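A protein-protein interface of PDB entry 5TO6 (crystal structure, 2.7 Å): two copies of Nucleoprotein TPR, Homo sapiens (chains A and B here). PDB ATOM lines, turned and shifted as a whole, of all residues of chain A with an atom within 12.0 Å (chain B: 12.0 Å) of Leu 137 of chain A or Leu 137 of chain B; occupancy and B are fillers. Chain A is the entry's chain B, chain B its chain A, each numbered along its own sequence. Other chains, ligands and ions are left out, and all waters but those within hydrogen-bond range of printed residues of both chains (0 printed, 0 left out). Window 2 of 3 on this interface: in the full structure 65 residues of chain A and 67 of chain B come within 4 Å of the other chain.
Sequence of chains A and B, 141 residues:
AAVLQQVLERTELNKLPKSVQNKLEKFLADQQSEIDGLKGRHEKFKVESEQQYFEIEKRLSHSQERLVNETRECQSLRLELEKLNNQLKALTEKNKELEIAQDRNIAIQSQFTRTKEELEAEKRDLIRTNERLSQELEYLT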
ATOM      1  N   ARG A 128      -0.315  11.976 -14.926  1.00  0.00           N
ATOM      2  CA  ARG A 128      -0.050  13.371 -15.243  1.00  0.00           C
ATOM      3  C   ARG A 128       1.280  13.834 -14.655  1.00  0.00           C
ATOM      4  O   ARG A 128       2.082  14.460 -15.346  1.00  0.00           O
ATOM      5  CB  ARG A 128      -1.194  14.245 -14.733  1.00  0.00           C
ATOM      6  CG  ARG A 128      -0.988  15.730 -14.932  1.00  0.00           C
ATOM      7  CD  ARG A 128      -2.274  16.494 -14.666  1.00  0.00           C
ATOM      8  NE  ARG A 128      -3.359  16.076 -15.552  1.00  0.00           N
ATOM      9  CZ  ARG A 128      -4.391  15.329 -15.171  1.00  0.00           C
ATOM     10  NH1 ARG A 128      -4.485  14.915 -13.915  1.00  0.00           N
ATOM     11  NH2 ARG A 128      -5.333  14.996 -16.046  1.00  0.00           N
ATOM     12  N   THR A 129       1.504  13.526 -13.381  1.00  0.00           N
ATOM     13  CA  THR A 129       2.771  13.829 -12.722  1.00  0.00           C
ATOM     14  C   THR A 129       3.894  13.024 -13.373  1.00  0.00           C
ATOM     15  O   THR A 129       5.024  13.496 -13.501  1.00  0.00           O
ATOM     16  CB  THR A 129       2.712  13.523 -11.212  1.00  0.00           C
ATOM     17  OG1 THR A 129       1.611  14.226 -10.621  1.00  0.00           O
ATOM     18  CG2 THR A 129       4.006  13.941 -10.522  1.00  0.00           C
ATOM     19  N   ASN A 130       3.564  11.803 -13.784  1.00  0.00           N
ATOM     20  CA  ASN A 130       4.506  10.927 -14.472  1.00  0.00           C
ATOM     21  C   ASN A 130       4.977  11.534 -15.788  1.00  0.00           C
ATOM     22  O   ASN A 130       6.159  11.466 -16.128  1.00  0.00           O
ATOM     23  CB  ASN A 130       3.875   9.556 -14.724  1.00  0.00           C
ATOM     24  CG  ASN A 130       4.902   8.488 -15.041  1.00  0.00           C
ATOM     25  OD1 ASN A 130       4.969   7.986 -16.163  1.00  0.00           O
ATOM     26  ND2 ASN A 130       5.708   8.130 -14.048  1.00  0.00           N
ATOM     27  N   GLU A 131       4.042  12.123 -16.527  1.00  0.00           N
ATOM     28  CA  GLU A 131       4.363  12.757 -17.799  1.00  0.00           C
ATOM     29  C   GLU A 131       5.225  13.998 -17.592  1.00  0.00           C
ATOM     30  O   GLU A 131       6.154  14.253 -18.360  1.00  0.00           O
ATOM     31  CB  GLU A 131       3.082  13.125 -18.550  1.00  0.00           C
ATOM     32  CG  GLU A 131       3.304  13.518 -20.001  1.00  0.00           C
ATOM     33  CD  GLU A 131       3.897  12.389 -20.824  1.00  0.00           C
ATOM     34  OE1 GLU A 131       3.121  11.587 -21.386  1.00  0.00           O
ATOM     35  OE2 GLU A 131       5.140  12.304 -20.911  1.00  0.00           O
ATOM     36  N   ARG A 132       4.910  14.772 -16.557  1.00  0.00           N
ATOM     37  CA  ARG A 132       5.696  15.954 -16.218  1.00  0.00           C
ATOM     38  C   ARG A 132       7.135  15.585 -15.864  1.00  0.00           C
ATOM     39  O   ARG A 132       8.078  16.229 -16.327  1.00  0.00           O
ATOM     40  CB  ARG A 132       5.041  16.730 -15.075  1.00  0.00           C
ATOM     41  CG  ARG A 132       5.862  17.909 -14.590  1.00  0.00           C
ATOM     42  CD  ARG A 132       5.114  18.705 -13.540  1.00  0.00           C
ATOM     43  NE  ARG A 132       3.727  18.937 -13.933  1.00  0.00           N
ATOM     44  CZ  ARG A 132       3.323  19.996 -14.628  1.00  0.00           C
ATOM     45  NH1 ARG A 132       4.201  20.917 -15.001  1.00  0.00           N
ATOM     46  NH2 ARG A 132       2.044  20.137 -14.950  1.00  0.00           N
ATOM     47  N   LEU A 133       7.296  14.550 -15.044  1.00  0.00           N
ATOM     48  CA  LEU A 133       8.623  14.070 -14.672  1.00  0.00           C
ATOM     49  C   LEU A 133       9.366  13.557 -15.898  1.00  0.00           C
ATOM     50  O   LEU A 133      10.581  13.712 -16.005  1.00  0.00           O
ATOM     51  CB  LEU A 133       8.529  12.966 -13.614  1.00  0.00           C
ATOM     52  CG  LEU A 133       8.097  13.388 -12.209  1.00  0.00           C
ATOM     53  CD1 LEU A 133       7.994  12.183 -11.289  1.00  0.00           C
ATOM     54  CD2 LEU A 133       9.064  14.415 -11.647  1.00  0.00           C
ATOM     55  N   SER A 134       8.628  12.942 -16.817  1.00  0.00           N
ATOM     56  CA  SER A 134       9.208  12.438 -18.057  1.00  0.00           C
ATOM     57  C   SER A 134       9.696  13.575 -18.954  1.00  0.00           C
ATOM     58  O   SER A 134      10.787  13.503 -19.522  1.00  0.00           O
ATOM     59  CB  SER A 134       8.192  11.580 -18.811  1.00  0.00           C
ATOM     60  OG  SER A 134       8.691  11.213 -20.084  1.00  0.00           O
ATOM     61  N   GLN A 135       8.879  14.618 -19.080  1.00  0.00           N
ATOM     62  CA  GLN A 135       9.225  15.775 -19.901  1.00  0.00           C
ATOM     63  C   GLN A 135      10.470  16.491 -19.391  1.00  0.00           C
ATOM     64  O   GLN A 135      11.339  16.877 -20.172  1.00  0.00           O
ATOM     65  CB  GLN A 135       8.055  16.765 -19.950  1.00  0.00           C
ATOM     66  CG  GLN A 135       6.879  16.330 -20.813  1.00  0.00           C
ATOM     67  CD  GLN A 135       7.275  16.065 -22.251  1.00  0.00           C
ATOM     68  OE1 GLN A 135       8.092  16.785 -22.827  1.00  0.00           O
ATOM     69  NE2 GLN A 135       6.688  15.032 -22.845  1.00  0.00           N
ATOM     70  N   GLU A 136      10.546  16.664 -18.076  1.00  0.00           N
ATOM     71  CA  GLU A 136      11.668  17.360 -17.462  1.00  0.00           C
ATOM     72  C   GLU A 136      12.947  16.525 -17.472  1.00  0.00           C
ATOM     73  O   GLU A 136      14.045  17.066 -17.601  1.00  0.00           O
ATOM     74  CB  GLU A 136      11.314  17.759 -16.026  1.00  0.00           C
ATOM     75  CG  GLU A 136      12.400  18.541 -15.305  1.00  0.00           C
ATOM     76  CD  GLU A 136      11.964  19.022 -13.936  1.00  0.00           C
ATOM     77  OE1 GLU A 136      10.798  18.770 -13.560  1.00  0.00           O
ATOM     78  OE2 GLU A 136      12.785  19.651 -13.236  1.00  0.00           O
ATOM     79  N   LEU A 137      12.807  15.209 -17.343  1.00  0.00           N
ATOM     80  CA  LEU A 137      13.972  14.328 -17.320  1.00  0.00           C
ATOM     81  C   LEU A 137      14.670  14.181 -18.673  1.00  0.00           C
ATOM     82  O   LEU A 137      15.886  14.346 -18.765  1.00  0.00           O
ATOM     83  CB  LEU A 137      13.566  12.945 -16.803  1.00  0.00           C
ATOM     84  CG  LEU A 137      14.705  12.029 -16.353  1.00  0.00           C
ATOM     85  CD1 LEU A 137      15.565  12.723 -15.308  1.00  0.00           C
ATOM     86  CD2 LEU A 137      14.154  10.720 -15.814  1.00  0.00           C
ATOM     87  N   GLU A 138      13.907  13.868 -19.718  1.00  0.00           N
ATOM     88  CA  GLU A 138      14.492  13.656 -21.042  1.00  0.00           C
ATOM     89  C   GLU A 138      15.073  14.922 -21.667  1.00  0.00           C
ATOM     90  O   GLU A 138      16.176  14.900 -22.215  1.00  0.00           O
ATOM     91  CB  GLU A 138      13.455  13.048 -21.991  1.00  0.00           C
ATOM     92  CG  GLU A 138      13.849  13.125 -23.462  1.00  0.00           C
ATOM     93  CD  GLU A 138      13.358  11.939 -24.270  1.00  0.00           C
ATOM     94  OE1 GLU A 138      12.630  12.152 -25.262  1.00  0.00           O
ATOM     95  OE2 GLU A 138      13.711  10.793 -23.919  1.00  0.00           O
ATOM     96  N   TYR A 139      14.341  16.027 -21.577  1.00  0.00           N
ATOM     97  CA  TYR A 139      14.800  17.281 -22.162  1.00  0.00           C
ATOM     98  C   TYR A 139      15.986  17.876 -21.415  1.00  0.00           C
ATOM     99  O   TYR A 139      16.968  18.298 -22.026  1.00  0.00           O
ATOM    100  CB  TYR A 139      13.651  18.293 -22.196  1.00  0.00           C
ATOM    101  CG  TYR A 139      14.017  19.640 -22.780  1.00  0.00           C
ATOM    102  CD1 TYR A 139      14.130  19.825 -24.151  1.00  0.00           C
ATOM    103  CD2 TYR A 139      14.242  20.733 -21.951  1.00  0.00           C
ATOM    104  CE1 TYR A 139      14.463  21.060 -24.680  1.00  0.00           C
ATOM    105  CE2 TYR A 139      14.574  21.969 -22.469  1.00  0.00           C
ATOM    106  CZ  TYR A 139      14.683  22.128 -23.833  1.00  0.00           C
ATOM    107  OH  TYR A 139      15.015  23.359 -24.350  1.00  0.00           O
ATOM    108  N   LEU A 140      15.887  17.908 -20.093  1.00  0.00           N
ATOM    109  CA  LEU A 140      16.949  18.462 -19.266  1.00  0.00           C
ATOM    110  C   LEU A 140      17.921  17.385 -18.794  1.00  0.00           C
ATOM    111  O   LEU A 140      18.785  16.939 -19.547  1.00  0.00           O
ATOM    112  CB  LEU A 140      16.348  19.214 -18.080  1.00  0.00           C
ATOM    113  CG  LEU A 140      15.710  20.534 -18.519  1.00  0.00           C
ATOM    114  CD1 LEU A 140      14.890  21.151 -17.397  1.00  0.00           C
ATOM    115  CD2 LEU A 140      16.764  21.509 -19.033  1.00  0.00           C
ATOM    116  N   ARG B 128       5.562   4.257  -7.715  1.00  0.00           N
ATOM    117  CA  ARG B 128       6.885   3.657  -7.816  1.00  0.00           C
ATOM    118  C   ARG B 128       7.698   4.280  -8.947  1.00  0.00           C
ATOM    119  O   ARG B 128       8.874   4.599  -8.775  1.00  0.00           O
ATOM    120  CB  ARG B 128       6.753   2.150  -8.030  1.00  0.00           C
ATOM    121  CG  ARG B 128       8.055   1.398  -8.202  1.00  0.00           C
ATOM    122  CD  ARG B 128       7.780  -0.099  -8.214  1.00  0.00           C
ATOM    123  NE  ARG B 128       8.983  -0.899  -8.417  1.00  0.00           N
ATOM    124  CZ  ARG B 128       9.761  -1.340  -7.434  1.00  0.00           C
ATOM    125  NH1 ARG B 128       9.467  -1.050  -6.174  1.00  0.00           N
ATOM    126  NH2 ARG B 128      10.834  -2.067  -7.710  1.00  0.00           N
ATOM    127  N   THR B 129       7.063   4.451 -10.104  1.00  0.00           N
ATOM    128  CA  THR B 129       7.729   5.018 -11.273  1.00  0.00           C
ATOM    129  C   THR B 129       8.051   6.501 -11.085  1.00  0.00           C
ATOM    130  O   THR B 129       9.124   6.960 -11.481  1.00  0.00           O
ATOM    131  CB  THR B 129       6.875   4.840 -12.546  1.00  0.00           C
ATOM    132  OG1 THR B 129       6.589   3.450 -12.737  1.00  0.00           O
ATOM    133  CG2 THR B 129       7.609   5.368 -13.769  1.00  0.00           C
ATOM    134  N   ASN B 130       7.132   7.243 -10.474  1.00  0.00           N
ATOM    135  CA  ASN B 130       7.377   8.653 -10.179  1.00  0.00           C
ATOM    136  C   ASN B 130       8.561   8.841  -9.240  1.00  0.00           C
ATOM    137  O   ASN B 130       9.338   9.782  -9.390  1.00  0.00           O
ATOM    138  CB  ASN B 130       6.130   9.306  -9.582  1.00  0.00           C
ATOM    139  CG  ASN B 130       5.125   9.710 -10.641  1.00  0.00           C
ATOM    140  OD1 ASN B 130       5.180   9.243 -11.779  1.00  0.00           O
ATOM    141  ND2 ASN B 130       4.207  10.595 -10.275  1.00  0.00           N
ATOM    142  N   GLU B 131       8.688   7.948  -8.264  1.00  0.00           N
ATOM    143  CA  GLU B 131       9.829   7.977  -7.359  1.00  0.00           C
ATOM    144  C   GLU B 131      11.123   7.755  -8.130  1.00  0.00           C
ATOM    145  O   GLU B 131      12.128   8.417  -7.877  1.00  0.00           O
ATOM    146  CB  GLU B 131       9.679   6.940  -6.245  1.00  0.00           C
ATOM    147  CG  GLU B 131      10.559   7.228  -5.036  1.00  0.00           C
ATOM    148  CD  GLU B 131      10.266   8.576  -4.399  1.00  0.00           C
ATOM    149  OE1 GLU B 131       9.089   8.991  -4.384  1.00  0.00           O
ATOM    150  OE2 GLU B 131      11.221   9.226  -3.920  1.00  0.00           O
ATOM    151  N   ARG B 132      11.094   6.805  -9.059  1.00  0.00           N
ATOM    152  CA  ARG B 132      12.255   6.516  -9.887  1.00  0.00           C
ATOM    153  C   ARG B 132      12.645   7.724 -10.725  1.00  0.00           C
ATOM    154  O   ARG B 132      13.820   8.069 -10.812  1.00  0.00           O
ATOM    155  CB  ARG B 132      11.979   5.325 -10.802  1.00  0.00           C
ATOM    156  CG  ARG B 132      13.086   5.044 -11.803  1.00  0.00           C
ATOM    157  CD  ARG B 132      12.551   4.236 -12.966  1.00  0.00           C
ATOM    158  NE  ARG B 132      11.697   3.144 -12.511  1.00  0.00           N
ATOM    159  CZ  ARG B 132      10.904   2.435 -13.309  1.00  0.00           C
ATOM    160  NH1 ARG B 132      10.853   2.710 -14.605  1.00  0.00           N
ATOM    161  NH2 ARG B 132      10.160   1.457 -12.811  1.00  0.00           N
ATOM    162  N   LEU B 133      11.653   8.374 -11.328  1.00  0.00           N
ATOM    163  CA  LEU B 133      11.906   9.545 -12.161  1.00  0.00           C
ATOM    164  C   LEU B 133      12.392  10.734 -11.341  1.00  0.00           C
ATOM    165  O   LEU B 133      13.242  11.501 -11.794  1.00  0.00           O
ATOM    166  CB  LEU B 133      10.651   9.936 -12.942  1.00  0.00           C
ATOM    167  CG  LEU B 133      10.103   8.884 -13.907  1.00  0.00           C
ATOM    168  CD1 LEU B 133       8.803   9.356 -14.540  1.00  0.00           C
ATOM    169  CD2 LEU B 133      11.135   8.546 -14.967  1.00  0.00           C
ATOM    170  N   SER B 134      11.850  10.884 -10.136  1.00  0.00           N
ATOM    171  CA  SER B 134      12.241  11.988  -9.270  1.00  0.00           C
ATOM    172  C   SER B 134      13.678  11.850  -8.771  1.00  0.00           C
ATOM    173  O   SER B 134      14.422  12.828  -8.740  1.00  0.00           O
ATOM    174  CB  SER B 134      11.286  12.093  -8.079  1.00  0.00           C
ATOM    175  OG  SER B 134      11.810  12.963  -7.091  1.00  0.00           O
ATOM    176  N   GLN B 135      14.055  10.641  -8.368  1.00  0.00           N
ATOM    177  CA  GLN B 135      15.408  10.379  -7.878  1.00  0.00           C
ATOM    178  C   GLN B 135      16.478  10.536  -8.960  1.00  0.00           C
ATOM    179  O   GLN B 135      17.562  11.057  -8.693  1.00  0.00           O
ATOM    180  CB  GLN B 135      15.487   8.985  -7.255  1.00  0.00           C
ATOM    181  CG  GLN B 135      14.919   8.929  -5.846  1.00  0.00           C
ATOM    182  CD  GLN B 135      15.045   7.562  -5.212  1.00  0.00           C
ATOM    183  OE1 GLN B 135      15.989   6.823  -5.490  1.00  0.00           O
ATOM    184  NE2 GLN B 135      14.100   7.222  -4.341  1.00  0.00           N
ATOM    185  N   GLU B 136      16.177  10.086 -10.174  1.00  0.00           N
ATOM    186  CA  GLU B 136      17.107  10.235 -11.290  1.00  0.00           C
ATOM    187  C   GLU B 136      17.261  11.707 -11.646  1.00  0.00           C
ATOM    188  O   GLU B 136      18.339  12.152 -12.038  1.00  0.00           O
ATOM    189  CB  GLU B 136      16.641   9.439 -12.512  1.00  0.00           C
ATOM    190  CG  GLU B 136      16.528   7.936 -12.287  1.00  0.00           C
ATOM    191  CD  GLU B 136      17.870   7.230 -12.346  1.00  0.00           C
ATOM    192  OE1 GLU B 136      18.858   7.865 -12.772  1.00  0.00           O
ATOM    193  OE2 GLU B 136      17.937   6.040 -11.973  1.00  0.00           O
ATOM    194  N   LEU B 137      16.174  12.457 -11.509  1.00  0.00           N
ATOM    195  CA  LEU B 137      16.179  13.885 -11.793  1.00  0.00           C
ATOM    196  C   LEU B 137      16.824  14.656 -10.645  1.00  0.00           C
ATOM    197  O   LEU B 137      17.420  15.715 -10.851  1.00  0.00           O
ATOM    198  CB  LEU B 137      14.751  14.381 -12.031  1.00  0.00           C
ATOM    199  CG  LEU B 137      14.527  15.845 -12.408  1.00  0.00           C
ATOM    200  CD1 LEU B 137      15.035  16.126 -13.814  1.00  0.00           C
ATOM    201  CD2 LEU B 137      13.051  16.190 -12.284  1.00  0.00           C
ATOM    202  N   GLU B 138      16.701  14.116  -9.437  1.00  0.00           N
ATOM    203  CA  GLU B 138      17.330  14.709  -8.263  1.00  0.00           C
ATOM    204  C   GLU B 138      18.848  14.593  -8.327  1.00  0.00           C
ATOM    205  O   GLU B 138      19.570  15.507  -7.926  1.00  0.00           O
ATOM    206  CB  GLU B 138      16.805  14.036  -6.991  1.00  0.00           C
ATOM    207  CG  GLU B 138      17.540  14.417  -5.720  1.00  0.00           C
ATOM    208  CD  GLU B 138      17.192  13.505  -4.558  1.00  0.00           C
ATOM    209  OE1 GLU B 138      16.280  12.662  -4.710  1.00  0.00           O
ATOM    210  OE2 GLU B 138      17.834  13.628  -3.494  1.00  0.00           O
ATOM    211  N   TYR B 139      19.325  13.470  -8.852  1.00  0.00           N
ATOM    212  CA  TYR B 139      20.756  13.225  -8.970  1.00  0.00           C
ATOM    213  C   TYR B 139      21.373  14.084 -10.067  1.00  0.00           C
ATOM    214  O   TYR B 139      22.489  14.586  -9.925  1.00  0.00           O
ATOM    215  CB  TYR B 139      21.018  11.743  -9.244  1.00  0.00           C
ATOM    216  CG  TYR B 139      22.468  11.395  -9.499  1.00  0.00           C
ATOM    217  CD1 TYR B 139      23.370  11.286  -8.450  1.00  0.00           C
ATOM    218  CD2 TYR B 139      22.930  11.158 -10.788  1.00  0.00           C
ATOM    219  CE1 TYR B 139      24.695  10.961  -8.677  1.00  0.00           C
ATOM    220  CE2 TYR B 139      24.253  10.832 -11.025  1.00  0.00           C
ATOM    221  CZ  TYR B 139      25.131  10.734  -9.967  1.00  0.00           C
ATOM    222  OH  TYR B 139      26.448  10.410 -10.202  1.00  0.00           O
ATOM    223  N   LEU B 140      20.639  14.244 -11.163  1.00  0.00           N
ATOM    224  CA  LEU B 140      21.149  14.974 -12.316  1.00  0.00           C
ATOM    225  C   LEU B 140      21.007  16.483 -12.131  1.00  0.00           C
ATOM    226  O   LEU B 140      21.644  17.265 -12.837  1.00  0.00           O
ATOM    227  CB  LEU B 140      20.425  14.529 -13.588  1.00  0.00           C
ATOM    228  CG  LEU B 140      20.908  13.211 -14.200  1.00  0.00           C
ATOM    229  CD1 LEU B 140      20.447  13.091 -15.644  1.00  0.00           C
ATOM    230  CD2 LEU B 140      22.420  13.070 -14.093  1.00  0.00           C
ATOM    231  N   THR B 141      20.168  16.888 -11.183  1.00  0.00           N
ATOM    232  CA  THR B 141      19.960  18.304 -10.895  1.00  0.00           C
ATOM    233  C   THR B 141      19.979  18.562  -9.390  1.00  0.00           C
ATOM    234  O   THR B 141      20.606  19.511  -8.917  1.00  0.00           O
ATOM    235  CB  THR B 141      18.633  18.814 -11.487  1.00  0.00           C
ATOM    236  OG1 THR B 141      18.669  18.696 -12.915  1.00  0.00           O
ATOM    237  CG2 THR B 141      18.405  20.272 -11.112  1.00  0.00           C
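The side-chain amide oxygen (OD1) of Asn 130 of chain B lies within hydrogen-bond range of the side-chain amide nitrogen (ND2) of Asn 130 of chain A, 2.6 Å away.
Among the printed residues, pairs that only touch across the chains: Leu 133 of chain A with Asn 130 of chain B, Thr 129 of chain A with Asn 130 of chain B, Asn 130 of chain A with Thr 129 of chain B, Asn 130 of chain A with Leu 133 of chain B, Glu 136 of chain A with Leu 137 of chain B, Leu 133 of chain A with Leu 133 of chain B, Leu 137 of chain A with Leu 137 of chain B and Leu 137 of chain A with Leu 133 of chain B.
Of chain B, only Leu 133 (3.8 Å) and Leu 137 (3.8 Å) come within 4 Å of Leu 137 of chain A.
Of chain A, only Glu 136 and Leu 137 come within 4 Å of Leu 137 of chain B.
No residue of chain B comes within 4 Å of Ser 134 of chain A.
Glu 136 of chain A touches just one residue of chain B: Leu 137 (3.5 Å).
No residue of chain B comes within 4 Å of Glu 138 of chain A.
No residue of chain A comes within 4 Å of Glu 136 of chain B.
No residue of chain A comes within 4 Å of Thr 141 of chain B.
Printed residues of chain B within 4 Å of Thr 129 of chain A: Asn 130 (3.4 Å).
Of the printed residues of chain A, Asn 130 of chain B touches Thr 129, Asn 130 and Leu 133.
Printed residues of chain B within 4 Å of Asn 130 of chain A: Thr 129, Asn 130 and Leu 133.
Of the printed residues of chain A, Thr 129 of chain B touches Asn 130.
Arg 128 of chain A touches none of the printed residues of chain B.
The nearest residue of chain B that does not touch Leu 137 of chain A is Glu 136 of chain B (4.2 Å).
Of the 13 printed residues of chain A, 5 touch a printed residue of chain B.
Printed residues of chain B that touch a printed residue of chain A: Thr 129, Asn 130, Leu 133 and Leu 137.
Among the printed residues, 9 pairs touch across the chains.
Among the printed residues, no Asp or Glu carboxylate lies within 4 Å of a Lys or Arg side-chain nitrogen of the other chain.
Thr 129 of chain A touches Asn 130 of chain B, and with the chains exchanged Asn 130 of chain A touches Thr 129 of chain B.
Asn 130 of chain B touches its own counterpart, Asn 130 of chain A.
Leu 137 of chain A touches Leu 133 of chain B, but with the chains exchanged Leu 133 of chain A does not touch Leu 137 of chain B (4.4 Å).
Leu 137 of chain B touches its own counterpart, Leu 137 of chain A.
Positions printed for both chains: 128, 129, 130, 131, 132, 133, 134, 135, 136, 137, 138, 139 and 140.
Of the 9 pairs that touch across the chains among the printed residues, 7 have their exchanged pair printed and touching as well.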
